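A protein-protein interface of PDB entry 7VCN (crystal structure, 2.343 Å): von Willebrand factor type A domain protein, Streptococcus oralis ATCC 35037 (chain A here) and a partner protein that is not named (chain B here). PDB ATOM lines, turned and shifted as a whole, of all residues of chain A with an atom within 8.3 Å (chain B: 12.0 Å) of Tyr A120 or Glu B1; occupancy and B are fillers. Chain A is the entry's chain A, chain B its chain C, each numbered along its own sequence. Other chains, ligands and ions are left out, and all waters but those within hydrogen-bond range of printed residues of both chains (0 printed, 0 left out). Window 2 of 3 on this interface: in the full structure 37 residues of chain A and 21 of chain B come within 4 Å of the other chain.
Of the 19 printed residues of chain A, 4 touch a printed residue of chain B. Hydrophobic or aromatic side chains of chain A within 4 Å of the printed part of chain B: Tyr A118 and Tyr A120. Of the 11 printed residues of chain B, 3 touch a printed residue of chain A. Printed residues of chain B that touch a printed residue of chain A: Glu B1, Thr B4 and Leu B6.
No residue of chain B comes within 4 Å of Gly A1. Tyr A120 touches just one residue of chain B: Glu B1 (3.5 Å). No residue of chain B comes within 4 Å of Gly A121. No residue of chain B comes within 4 Å of Gly A123. No residue of chain B comes within 4 Å of Gln A126. No residue of chain B comes within 4 Å of Thr A127. Of the printed residues of chain B, Lys A128 touches Glu B1. Of the printed residues of chain B, Lys A130 touches Thr B4 (3.1 Å) and Leu B6 (3.7 Å). Of chain A, only Tyr A120 (3.5 Å) and Lys A128 (3.1 Å) come within 4 Å of Glu B1. Of the printed residues of chain A, Thr B4 touches Tyr A118 (3.2 Å) and Lys A130 (3.1 Å). Of the printed residues of chain A, Leu B6 touches Lys A130. Thr B27 touches none of the printed residues of chain A. The nearest residue of chain B that does not touch Tyr A120 is Pro B2 (4.5 Å). The nearest residue of chain A that does not touch Glu B1 is Tyr A118 (4.7 Å). The nearest printed residue of chain A that does not touch Thr B4 is Ile A2 (4.1 Å).
OE1 of Glu B1 lies within salt-bridge range of NZ of Lys A128. The side-chain hydroxyl of Thr B4 is in hydrogen-bond range of the side-chain hydroxyl of Tyr A118. OG1 of Thr B4 lies within hydrogen-bond range of NZ of Lys A130.
Among the printed residues, merely in contact across the chains: Tyr A120 with Glu B1 and Lys A130 with Leu B6.
The backbone carbonyl oxygen (O) of Glu B1 is in hydrogen-bond range of the side-chain amide nitrogen (NE2) of Gln B3 (3.2 Å). O of Tyr A118 lies within hydrogen-bond range of N of Lys A128 (3.0 Å). The backbone NH (N) of Gln A126 sits at hydrogen-bond distance from the backbone carbonyl oxygen (O) of Tyr A120.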
ATOM      1  N   GLY A   1     -26.854  13.327   5.355  1.00  0.00           N
ATOM      2  CA  GLY A   1     -25.746  14.115   4.761  1.00  0.00           C
ATOM      3  C   GLY A   1     -25.322  15.266   5.686  1.00  0.00           C
ATOM      4  O   GLY A   1     -26.054  15.621   6.629  1.00  0.00           O
ATOM      5  N   ILE A   2     -24.136  15.861   5.445  1.00  0.00           N
ATOM      6  CA  ILE A   2     -23.849  17.110   6.157  1.00  0.00           C
ATOM      7  C   ILE A   2     -24.364  18.291   5.316  1.00  0.00           C
ATOM      8  O   ILE A   2     -24.419  18.200   4.077  1.00  0.00           O
ATOM      9  CB  ILE A   2     -22.380  17.255   6.611  1.00  0.00           C
ATOM     10  CG1 ILE A   2     -21.503  17.791   5.474  1.00  0.00           C
ATOM     11  CG2 ILE A   2     -21.841  15.953   7.195  1.00  0.00           C
ATOM     12  CD1 ILE A   2     -20.023  17.811   5.764  1.00  0.00           C
ATOM     13  N   HIS A   3     -24.793  19.366   5.994  1.00  0.00           N
ATOM     14  CA  HIS A   3     -25.319  20.525   5.279  1.00  0.00           C
ATOM     15  C   HIS A   3     -24.810  21.828   5.923  1.00  0.00           C
ATOM     16  O   HIS A   3     -24.010  21.797   6.875  1.00  0.00           O
ATOM     17  CB  HIS A   3     -26.844  20.417   5.127  1.00  0.00           C
ATOM     18  CG  HIS A   3     -27.523  20.107   6.436  1.00  0.00           C
ATOM     19  ND1 HIS A   3     -27.907  21.100   7.342  1.00  0.00           N
ATOM     20  CD2 HIS A   3     -27.803  18.932   7.052  1.00  0.00           C
ATOM     21  CE1 HIS A   3     -28.403  20.555   8.428  1.00  0.00           C
ATOM     22  NE2 HIS A   3     -28.348  19.237   8.280  1.00  0.00           N
ATOM     23  N   HIS A   4     -25.306  22.958   5.388  1.00  0.00           N
ATOM     24  CA  HIS A   4     -24.892  24.281   5.829  1.00  0.00           C
ATOM     25  C   HIS A   4     -23.372  24.344   5.764  1.00  0.00           C
ATOM     26  O   HIS A   4     -22.721  24.707   6.731  1.00  0.00           O
ATOM     27  CB  HIS A   4     -25.484  24.608   7.228  1.00  0.00           C
ATOM     28  CG  HIS A   4     -26.972  24.833   7.137  1.00  0.00           C
ATOM     29  ND1 HIS A   4     -27.906  23.789   7.245  1.00  0.00           N
ATOM     30  CD2 HIS A   4     -27.700  25.945   6.853  1.00  0.00           C
ATOM     31  CE1 HIS A   4     -29.109  24.260   7.049  1.00  0.00           C
ATOM     32  NE2 HIS A   4     -29.010  25.563   6.819  1.00  0.00           N
ATOM     33  N   VAL A   5     -22.804  23.850   4.672  1.00  0.00           N
ATOM     34  CA  VAL A   5     -21.371  23.599   4.670  1.00  0.00           C
ATOM     35  C   VAL A   5     -20.647  24.887   4.272  1.00  0.00           C
ATOM     36  O   VAL A   5     -21.127  25.659   3.449  1.00  0.00           O
ATOM     37  CB  VAL A   5     -21.020  22.468   3.703  1.00  0.00           C
ATOM     38  CG1 VAL A   5     -19.532  22.301   3.586  1.00  0.00           C
ATOM     39  CG2 VAL A   5     -21.641  21.160   4.165  1.00  0.00           C
ATOM     40  N   THR A 117     -16.867  24.530   8.426  1.00  0.00           N
ATOM     41  CA  THR A 117     -18.031  24.511   9.299  1.00  0.00           C
ATOM     42  C   THR A 117     -19.169  23.748   8.627  1.00  0.00           C
ATOM     43  O   THR A 117     -19.409  23.909   7.418  1.00  0.00           O
ATOM     44  CB  THR A 117     -18.505  25.928   9.622  1.00  0.00           C
ATOM     45  OG1 THR A 117     -17.514  26.359  10.548  1.00  0.00           O
ATOM     46  CG2 THR A 117     -19.810  25.920  10.390  1.00  0.00           C
ATOM     47  N   TYR A 118     -19.859  22.934   9.425  1.00  0.00           N
ATOM     48  CA  TYR A 118     -20.984  22.181   8.887  1.00  0.00           C
ATOM     49  C   TYR A 118     -21.975  21.779   9.982  1.00  0.00           C
ATOM     50  O   TYR A 118     -21.651  21.673  11.176  1.00  0.00           O
ATOM     51  CB  TYR A 118     -20.527  20.962   8.069  1.00  0.00           C
ATOM     52  CG  TYR A 118     -19.724  19.930   8.824  1.00  0.00           C
ATOM     53  CD1 TYR A 118     -18.335  20.018   8.897  1.00  0.00           C
ATOM     54  CD2 TYR A 118     -20.335  18.878   9.503  1.00  0.00           C
ATOM     55  CE1 TYR A 118     -17.580  19.090   9.622  1.00  0.00           C
ATOM     56  CE2 TYR A 118     -19.599  17.956  10.239  1.00  0.00           C
ATOM     57  CZ  TYR A 118     -18.222  18.050  10.286  1.00  0.00           C
ATOM     58  OH  TYR A 118     -17.521  17.133  10.995  1.00  0.00           O
ATOM     59  N   SER A 119     -23.184  21.511   9.498  1.00  0.00           N
ATOM     60  CA  SER A 119     -24.248  21.002  10.340  1.00  0.00           C
ATOM     61  C   SER A 119     -24.657  19.600   9.896  1.00  0.00           C
ATOM     62  O   SER A 119     -24.392  19.200   8.758  1.00  0.00           O
ATOM     63  CB  SER A 119     -25.372  21.951  10.287  1.00  0.00           C
ATOM     64  OG  SER A 119     -24.972  23.096  10.984  1.00  0.00           O
ATOM     65  N   TYR A 120     -25.304  18.875  10.815  1.00  0.00           N
ATOM     66  CA  TYR A 120     -25.857  17.559  10.508  1.00  0.00           C
ATOM     67  C   TYR A 120     -27.011  17.255  11.451  1.00  0.00           C
ATOM     68  O   TYR A 120     -26.993  17.679  12.610  1.00  0.00           O
ATOM     69  CB  TYR A 120     -24.806  16.458  10.642  1.00  0.00           C
ATOM     70  CG  TYR A 120     -24.190  16.378  12.015  1.00  0.00           C
ATOM     71  CD1 TYR A 120     -23.168  17.243  12.397  1.00  0.00           C
ATOM     72  CD2 TYR A 120     -24.647  15.462  12.946  1.00  0.00           C
ATOM     73  CE1 TYR A 120     -22.591  17.182  13.657  1.00  0.00           C
ATOM     74  CE2 TYR A 120     -24.077  15.381  14.205  1.00  0.00           C
ATOM     75  CZ  TYR A 120     -23.050  16.239  14.562  1.00  0.00           C
ATOM     76  OH  TYR A 120     -22.502  16.132  15.802  1.00  0.00           O
ATOM     77  N   GLY A 121     -27.997  16.532  10.913  1.00  0.00           N
ATOM     78  CA  GLY A 121     -29.202  16.267  11.658  1.00  0.00           C
ATOM     79  C   GLY A 121     -30.379  16.967  10.999  1.00  0.00           C
ATOM     80  O   GLY A 121     -30.211  17.950  10.297  1.00  0.00           O
ATOM     81  N   ILE A 122     -31.561  16.390  11.194  1.00  0.00           N
ATOM     82  CA  ILE A 122     -32.822  17.050  10.911  1.00  0.00           C
ATOM     83  C   ILE A 122     -33.185  17.833  12.178  1.00  0.00           C
ATOM     84  O   ILE A 122     -32.512  17.685  13.208  1.00  0.00           O
ATOM     85  CB  ILE A 122     -33.919  16.057  10.436  1.00  0.00           C
ATOM     86  CG1 ILE A 122     -34.177  14.943  11.469  1.00  0.00           C
ATOM     87  CG2 ILE A 122     -33.580  15.515   9.050  1.00  0.00           C
ATOM     88  CD1 ILE A 122     -35.646  14.588  11.753  1.00  0.00           C
ATOM     89  N   GLY A 123     -34.190  18.714  12.051  1.00  0.00           N
ATOM     90  CA  GLY A 123     -34.659  19.542  13.146  1.00  0.00           C
ATOM     91  C   GLY A 123     -33.537  20.436  13.636  1.00  0.00           C
ATOM     92  O   GLY A 123     -32.816  20.981  12.824  1.00  0.00           O
ATOM     93  N   ASN A 124     -33.378  20.558  14.955  1.00  0.00           N
ATOM     94  CA  ASN A 124     -32.240  21.307  15.459  1.00  0.00           C
ATOM     95  C   ASN A 124     -30.979  20.498  15.209  1.00  0.00           C
ATOM     96  O   ASN A 124     -30.573  19.698  16.050  1.00  0.00           O
ATOM     97  CB  ASN A 124     -32.311  21.619  16.948  1.00  0.00           C
ATOM     98  CG  ASN A 124     -33.407  22.579  17.317  1.00  0.00           C
ATOM     99  OD1 ASN A 124     -34.084  22.357  18.309  1.00  0.00           O
ATOM    100  ND2 ASN A 124     -33.563  23.657  16.568  1.00  0.00           N
ATOM    101  N   SER A 125     -30.369  20.725  14.055  1.00  0.00           N
ATOM    102  CA  SER A 125     -29.132  20.058  13.704  1.00  0.00           C
ATOM    103  C   SER A 125     -28.008  20.384  14.716  1.00  0.00           C
ATOM    104  O   SER A 125     -28.236  21.076  15.715  1.00  0.00           O
ATOM    105  CB  SER A 125     -28.821  20.386  12.269  1.00  0.00           C
ATOM    106  OG  SER A 125     -28.702  21.788  12.086  1.00  0.00           O
ATOM    107  N   GLN A 126     -26.807  19.804  14.539  1.00  0.00           N
ATOM    108  CA  GLN A 126     -25.660  20.165  15.367  1.00  0.00           C
ATOM    109  C   GLN A 126     -24.574  20.751  14.477  1.00  0.00           C
ATOM    110  O   GLN A 126     -24.521  20.429  13.287  1.00  0.00           O
ATOM    111  CB  GLN A 126     -25.071  18.959  16.084  1.00  0.00           C
ATOM    112  CG  GLN A 126     -26.132  18.057  16.694  1.00  0.00           C
ATOM    113  CD  GLN A 126     -25.617  17.300  17.893  1.00  0.00           C
ATOM    114  OE1 GLN A 126     -24.921  17.847  18.751  1.00  0.00           O
ATOM    115  NE2 GLN A 126     -25.975  16.026  17.960  1.00  0.00           N
ATOM    116  N   THR A 127     -23.731  21.588  15.084  1.00  0.00           N
ATOM    117  CA  THR A 127     -22.713  22.302  14.340  1.00  0.00           C
ATOM    118  C   THR A 127     -21.316  21.942  14.836  1.00  0.00           C
ATOM    119  O   THR A 127     -21.078  21.985  16.027  1.00  0.00           O
ATOM    120  CB  THR A 127     -22.952  23.818  14.353  1.00  0.00           C
ATOM    121  OG1 THR A 127     -24.137  23.963  13.572  1.00  0.00           O
ATOM    122  CG2 THR A 127     -21.821  24.607  13.722  1.00  0.00           C
ATOM    123  N   LYS A 128     -20.408  21.626  13.902  1.00  0.00           N
ATOM    124  CA  LYS A 128     -18.994  21.437  14.158  1.00  0.00           C
ATOM    125  C   LYS A 128     -18.169  22.408  13.304  1.00  0.00           C
ATOM    126  O   LYS A 128     -18.525  22.718  12.168  1.00  0.00           O
ATOM    127  CB  LYS A 128     -18.616  20.068  13.609  1.00  0.00           C
ATOM    128  CG  LYS A 128     -18.896  18.861  14.482  1.00  0.00           C
ATOM    129  CD  LYS A 128     -17.639  18.123  14.929  1.00  0.00           C
ATOM    130  CE  LYS A 128     -17.982  16.978  15.872  1.00  0.00           C
ATOM    131  NZ  LYS A 128     -18.938  17.453  16.909  1.00  0.00           N
ATOM    132  N   THR A 129     -17.008  22.810  13.825  1.00  0.00           N
ATOM    133  CA  THR A 129     -15.923  23.357  13.017  1.00  0.00           C
ATOM    134  C   THR A 129     -14.674  22.476  13.146  1.00  0.00           C
ATOM    135  O   THR A 129     -14.316  22.127  14.257  1.00  0.00           O
ATOM    136  CB  THR A 129     -15.634  24.794  13.448  1.00  0.00           C
ATOM    137  OG1 THR A 129     -16.827  25.509  13.147  1.00  0.00           O
ATOM    138  CG2 THR A 129     -14.524  25.411  12.635  1.00  0.00           C
ATOM    139  N   LYS A 130     -14.045  22.072  12.034  1.00  0.00           N
ATOM    140  CA  LYS A 130     -12.770  21.395  12.094  1.00  0.00           C
ATOM    141  C   LYS A 130     -11.747  22.290  11.427  1.00  0.00           C
ATOM    142  O   LYS A 130     -12.020  22.759  10.323  1.00  0.00           O
ATOM    143  CB  LYS A 130     -12.784  20.069  11.341  1.00  0.00           C
ATOM    144  CG  LYS A 130     -13.555  18.985  12.058  1.00  0.00           C
ATOM    145  CD  LYS A 130     -13.841  17.772  11.218  1.00  0.00           C
ATOM    146  CE  LYS A 130     -12.746  16.739  11.301  1.00  0.00           C
ATOM    147  NZ  LYS A 130     -13.403  15.423  11.453  1.00  0.00           N
ATOM    148  N   GLU B   1     -22.978  11.409  14.085  1.00  0.00           N
ATOM    149  CA  GLU B   1     -22.275  12.276  13.079  1.00  0.00           C
ATOM    150  C   GLU B   1     -21.495  11.437  12.081  1.00  0.00           C
ATOM    151  O   GLU B   1     -20.723  10.564  12.481  1.00  0.00           O
ATOM    152  CB  GLU B   1     -21.277  13.260  13.694  1.00  0.00           C
ATOM    153  CG  GLU B   1     -20.404  12.693  14.794  1.00  0.00           C
ATOM    154  CD  GLU B   1     -19.415  13.691  15.373  1.00  0.00           C
ATOM    155  OE1 GLU B   1     -19.446  13.914  16.607  1.00  0.00           O
ATOM    156  OE2 GLU B   1     -18.605  14.245  14.590  1.00  0.00           O
ATOM    157  N   PRO B   2     -21.644  11.712  10.760  1.00  0.00           N
ATOM    158  CA  PRO B   2     -20.729  11.185   9.742  1.00  0.00           C
ATOM    159  C   PRO B   2     -19.275  11.628   9.956  1.00  0.00           C
ATOM    160  O   PRO B   2     -18.982  12.601  10.649  1.00  0.00           O
ATOM    161  CB  PRO B   2     -21.322  11.664   8.403  1.00  0.00           C
ATOM    162  CG  PRO B   2     -22.768  11.981   8.723  1.00  0.00           C
ATOM    163  CD  PRO B   2     -22.729  12.495  10.156  1.00  0.00           C
ATOM    164  N   GLN B   3     -18.366  10.813   9.424  1.00  0.00           N
ATOM    165  CA  GLN B   3     -16.956  11.087   9.492  1.00  0.00           C
ATOM    166  C   GLN B   3     -16.626  12.062   8.375  1.00  0.00           C
ATOM    167  O   GLN B   3     -17.132  11.920   7.266  1.00  0.00           O
ATOM    168  CB  GLN B   3     -16.198   9.765   9.336  1.00  0.00           C
ATOM    169  CG  GLN B   3     -16.465   8.740  10.443  1.00  0.00           C
ATOM    170  CD  GLN B   3     -16.756   9.284  11.830  1.00  0.00           C
ATOM    171  OE1 GLN B   3     -15.948   9.981  12.449  1.00  0.00           O
ATOM    172  NE2 GLN B   3     -17.926   8.951  12.355  1.00  0.00           N
ATOM    173  N   THR B   4     -15.786  13.056   8.678  1.00  0.00           N
ATOM    174  CA  THR B   4     -15.310  13.956   7.641  1.00  0.00           C
ATOM    175  C   THR B   4     -13.794  13.922   7.609  1.00  0.00           C
ATOM    176  O   THR B   4     -13.175  13.791   8.651  1.00  0.00           O
ATOM    177  CB  THR B   4     -15.832  15.376   7.837  1.00  0.00           C
ATOM    178  OG1 THR B   4     -15.357  15.781   9.124  1.00  0.00           O
ATOM    179  CG2 THR B   4     -17.345  15.446   7.744  1.00  0.00           C
ATOM    180  N   THR B   5     -13.228  13.984   6.405  1.00  0.00           N
ATOM    181  CA  THR B   5     -11.794  14.176   6.303  1.00  0.00           C
ATOM    182  C   THR B   5     -11.518  15.459   5.527  1.00  0.00           C
ATOM    183  O   THR B   5     -12.320  15.851   4.692  1.00  0.00           O
ATOM    184  CB  THR B   5     -11.084  12.929   5.767  1.00  0.00           C
ATOM    185  OG1 THR B   5     -11.582  12.743   4.441  1.00  0.00           O
ATOM    186  CG2 THR B   5     -11.327  11.703   6.616  1.00  0.00           C
ATOM    187  N   LEU B   6     -10.380  16.090   5.812  1.00  0.00           N
ATOM    188  CA  LEU B   6     -10.069  17.428   5.349  1.00  0.00           C
ATOM    189  C   LEU B   6      -8.640  17.430   4.872  1.00  0.00           C
ATOM    190  O   LEU B   6      -7.779  17.034   5.647  1.00  0.00           O
ATOM    191  CB  LEU B   6     -10.034  18.307   6.589  1.00  0.00           C
ATOM    192  CG  LEU B   6     -11.291  19.075   6.913  1.00  0.00           C
ATOM    193  CD1 LEU B   6     -12.307  18.080   7.447  1.00  0.00           C
ATOM    194  CD2 LEU B   6     -10.953  20.097   7.980  1.00  0.00           C
ATOM    195  N   ILE B  26     -13.087  18.619   1.513  1.00  0.00           N
ATOM    196  CA  ILE B  26     -13.868  17.967   2.556  1.00  0.00           C
ATOM    197  C   ILE B  26     -14.490  16.725   1.905  1.00  0.00           C
ATOM    198  O   ILE B  26     -14.913  16.785   0.744  1.00  0.00           O
ATOM    199  CB  ILE B  26     -14.981  18.902   3.106  1.00  0.00           C
ATOM    200  CG1 ILE B  26     -15.985  18.165   3.973  1.00  0.00           C
ATOM    201  CG2 ILE B  26     -15.731  19.588   1.996  1.00  0.00           C
ATOM    202  CD1 ILE B  26     -15.834  18.469   5.422  1.00  0.00           C
ATOM    203  N   THR B  27     -14.530  15.610   2.642  1.00  0.00           N
ATOM    204  CA  THR B  27     -15.213  14.402   2.198  1.00  0.00           C
ATOM    205  C   THR B  27     -16.070  13.922   3.353  1.00  0.00           C
ATOM    206  O   THR B  27     -15.564  13.851   4.469  1.00  0.00           O
ATOM    207  CB  THR B  27     -14.230  13.270   1.891  1.00  0.00           C
ATOM    208  OG1 THR B  27     -13.384  13.763   0.873  1.00  0.00           O
ATOM    209  CG2 THR B  27     -14.900  12.037   1.323  1.00  0.00           C
ATOM    210  N   SER B  28     -17.345  13.612   3.086  1.00  0.00           N
ATOM    211  CA  SER B  28     -18.150  13.048   4.160  1.00  0.00           C
ATOM    212  C   SER B  28     -18.402  11.559   3.921  1.00  0.00           C
ATOM    213  O   SER B  28     -18.574  11.178   2.770  1.00  0.00           O
ATOM    214  CB  SER B  28     -19.416  13.791   4.305  1.00  0.00           C
ATOM    215  OG  SER B  28     -20.383  12.972   4.933  1.00  0.00           O
ATOM    216  N   LYS B  29     -18.409  10.747   4.997  1.00  0.00           N
ATOM    217  CA  LYS B  29     -18.539   9.288   4.944  1.00  0.00           C
ATOM    218  C   LYS B  29     -19.562   8.784   5.957  1.00  0.00           C
ATOM    219  O   LYS B  29     -19.587   9.270   7.089  1.00  0.00           O
ATOM    220  CB  LYS B  29     -17.209   8.646   5.359  1.00  0.00           C
ATOM    221  CG  LYS B  29     -16.077   8.729   4.343  1.00  0.00           C
ATOM    222  CD  LYS B  29     -16.413   8.010   3.032  1.00  0.00           C
ATOM    223  CE  LYS B  29     -16.660   6.516   3.160  1.00  0.00           C
ATOM    224  NZ  LYS B  29     -17.901   6.074   2.473  1.00  0.00           N
ATOM    225  N   LEU B  30     -20.348   7.763   5.573  1.00  0.00           N
ATOM    226  CA  LEU B  30     -21.327   7.124   6.454  1.00  0.00           C
ATOM    227  C   LEU B  30     -20.801   5.747   6.885  1.00  0.00           C
ATOM    228  O   LEU B  30     -20.081   5.740   7.899  1.00  0.00           O
ATOM    229  CB  LEU B  30     -22.699   7.018   5.766  1.00  0.00           C
ATOM    230  CG  LEU B  30     -23.715   8.096   6.146  1.00  0.00           C
ATOM    231  CD1 LEU B  30     -23.850   8.182   7.666  1.00  0.00           C
ATOM    232  CD2 LEU B  30     -23.351   9.454   5.540  1.00  0.00           C
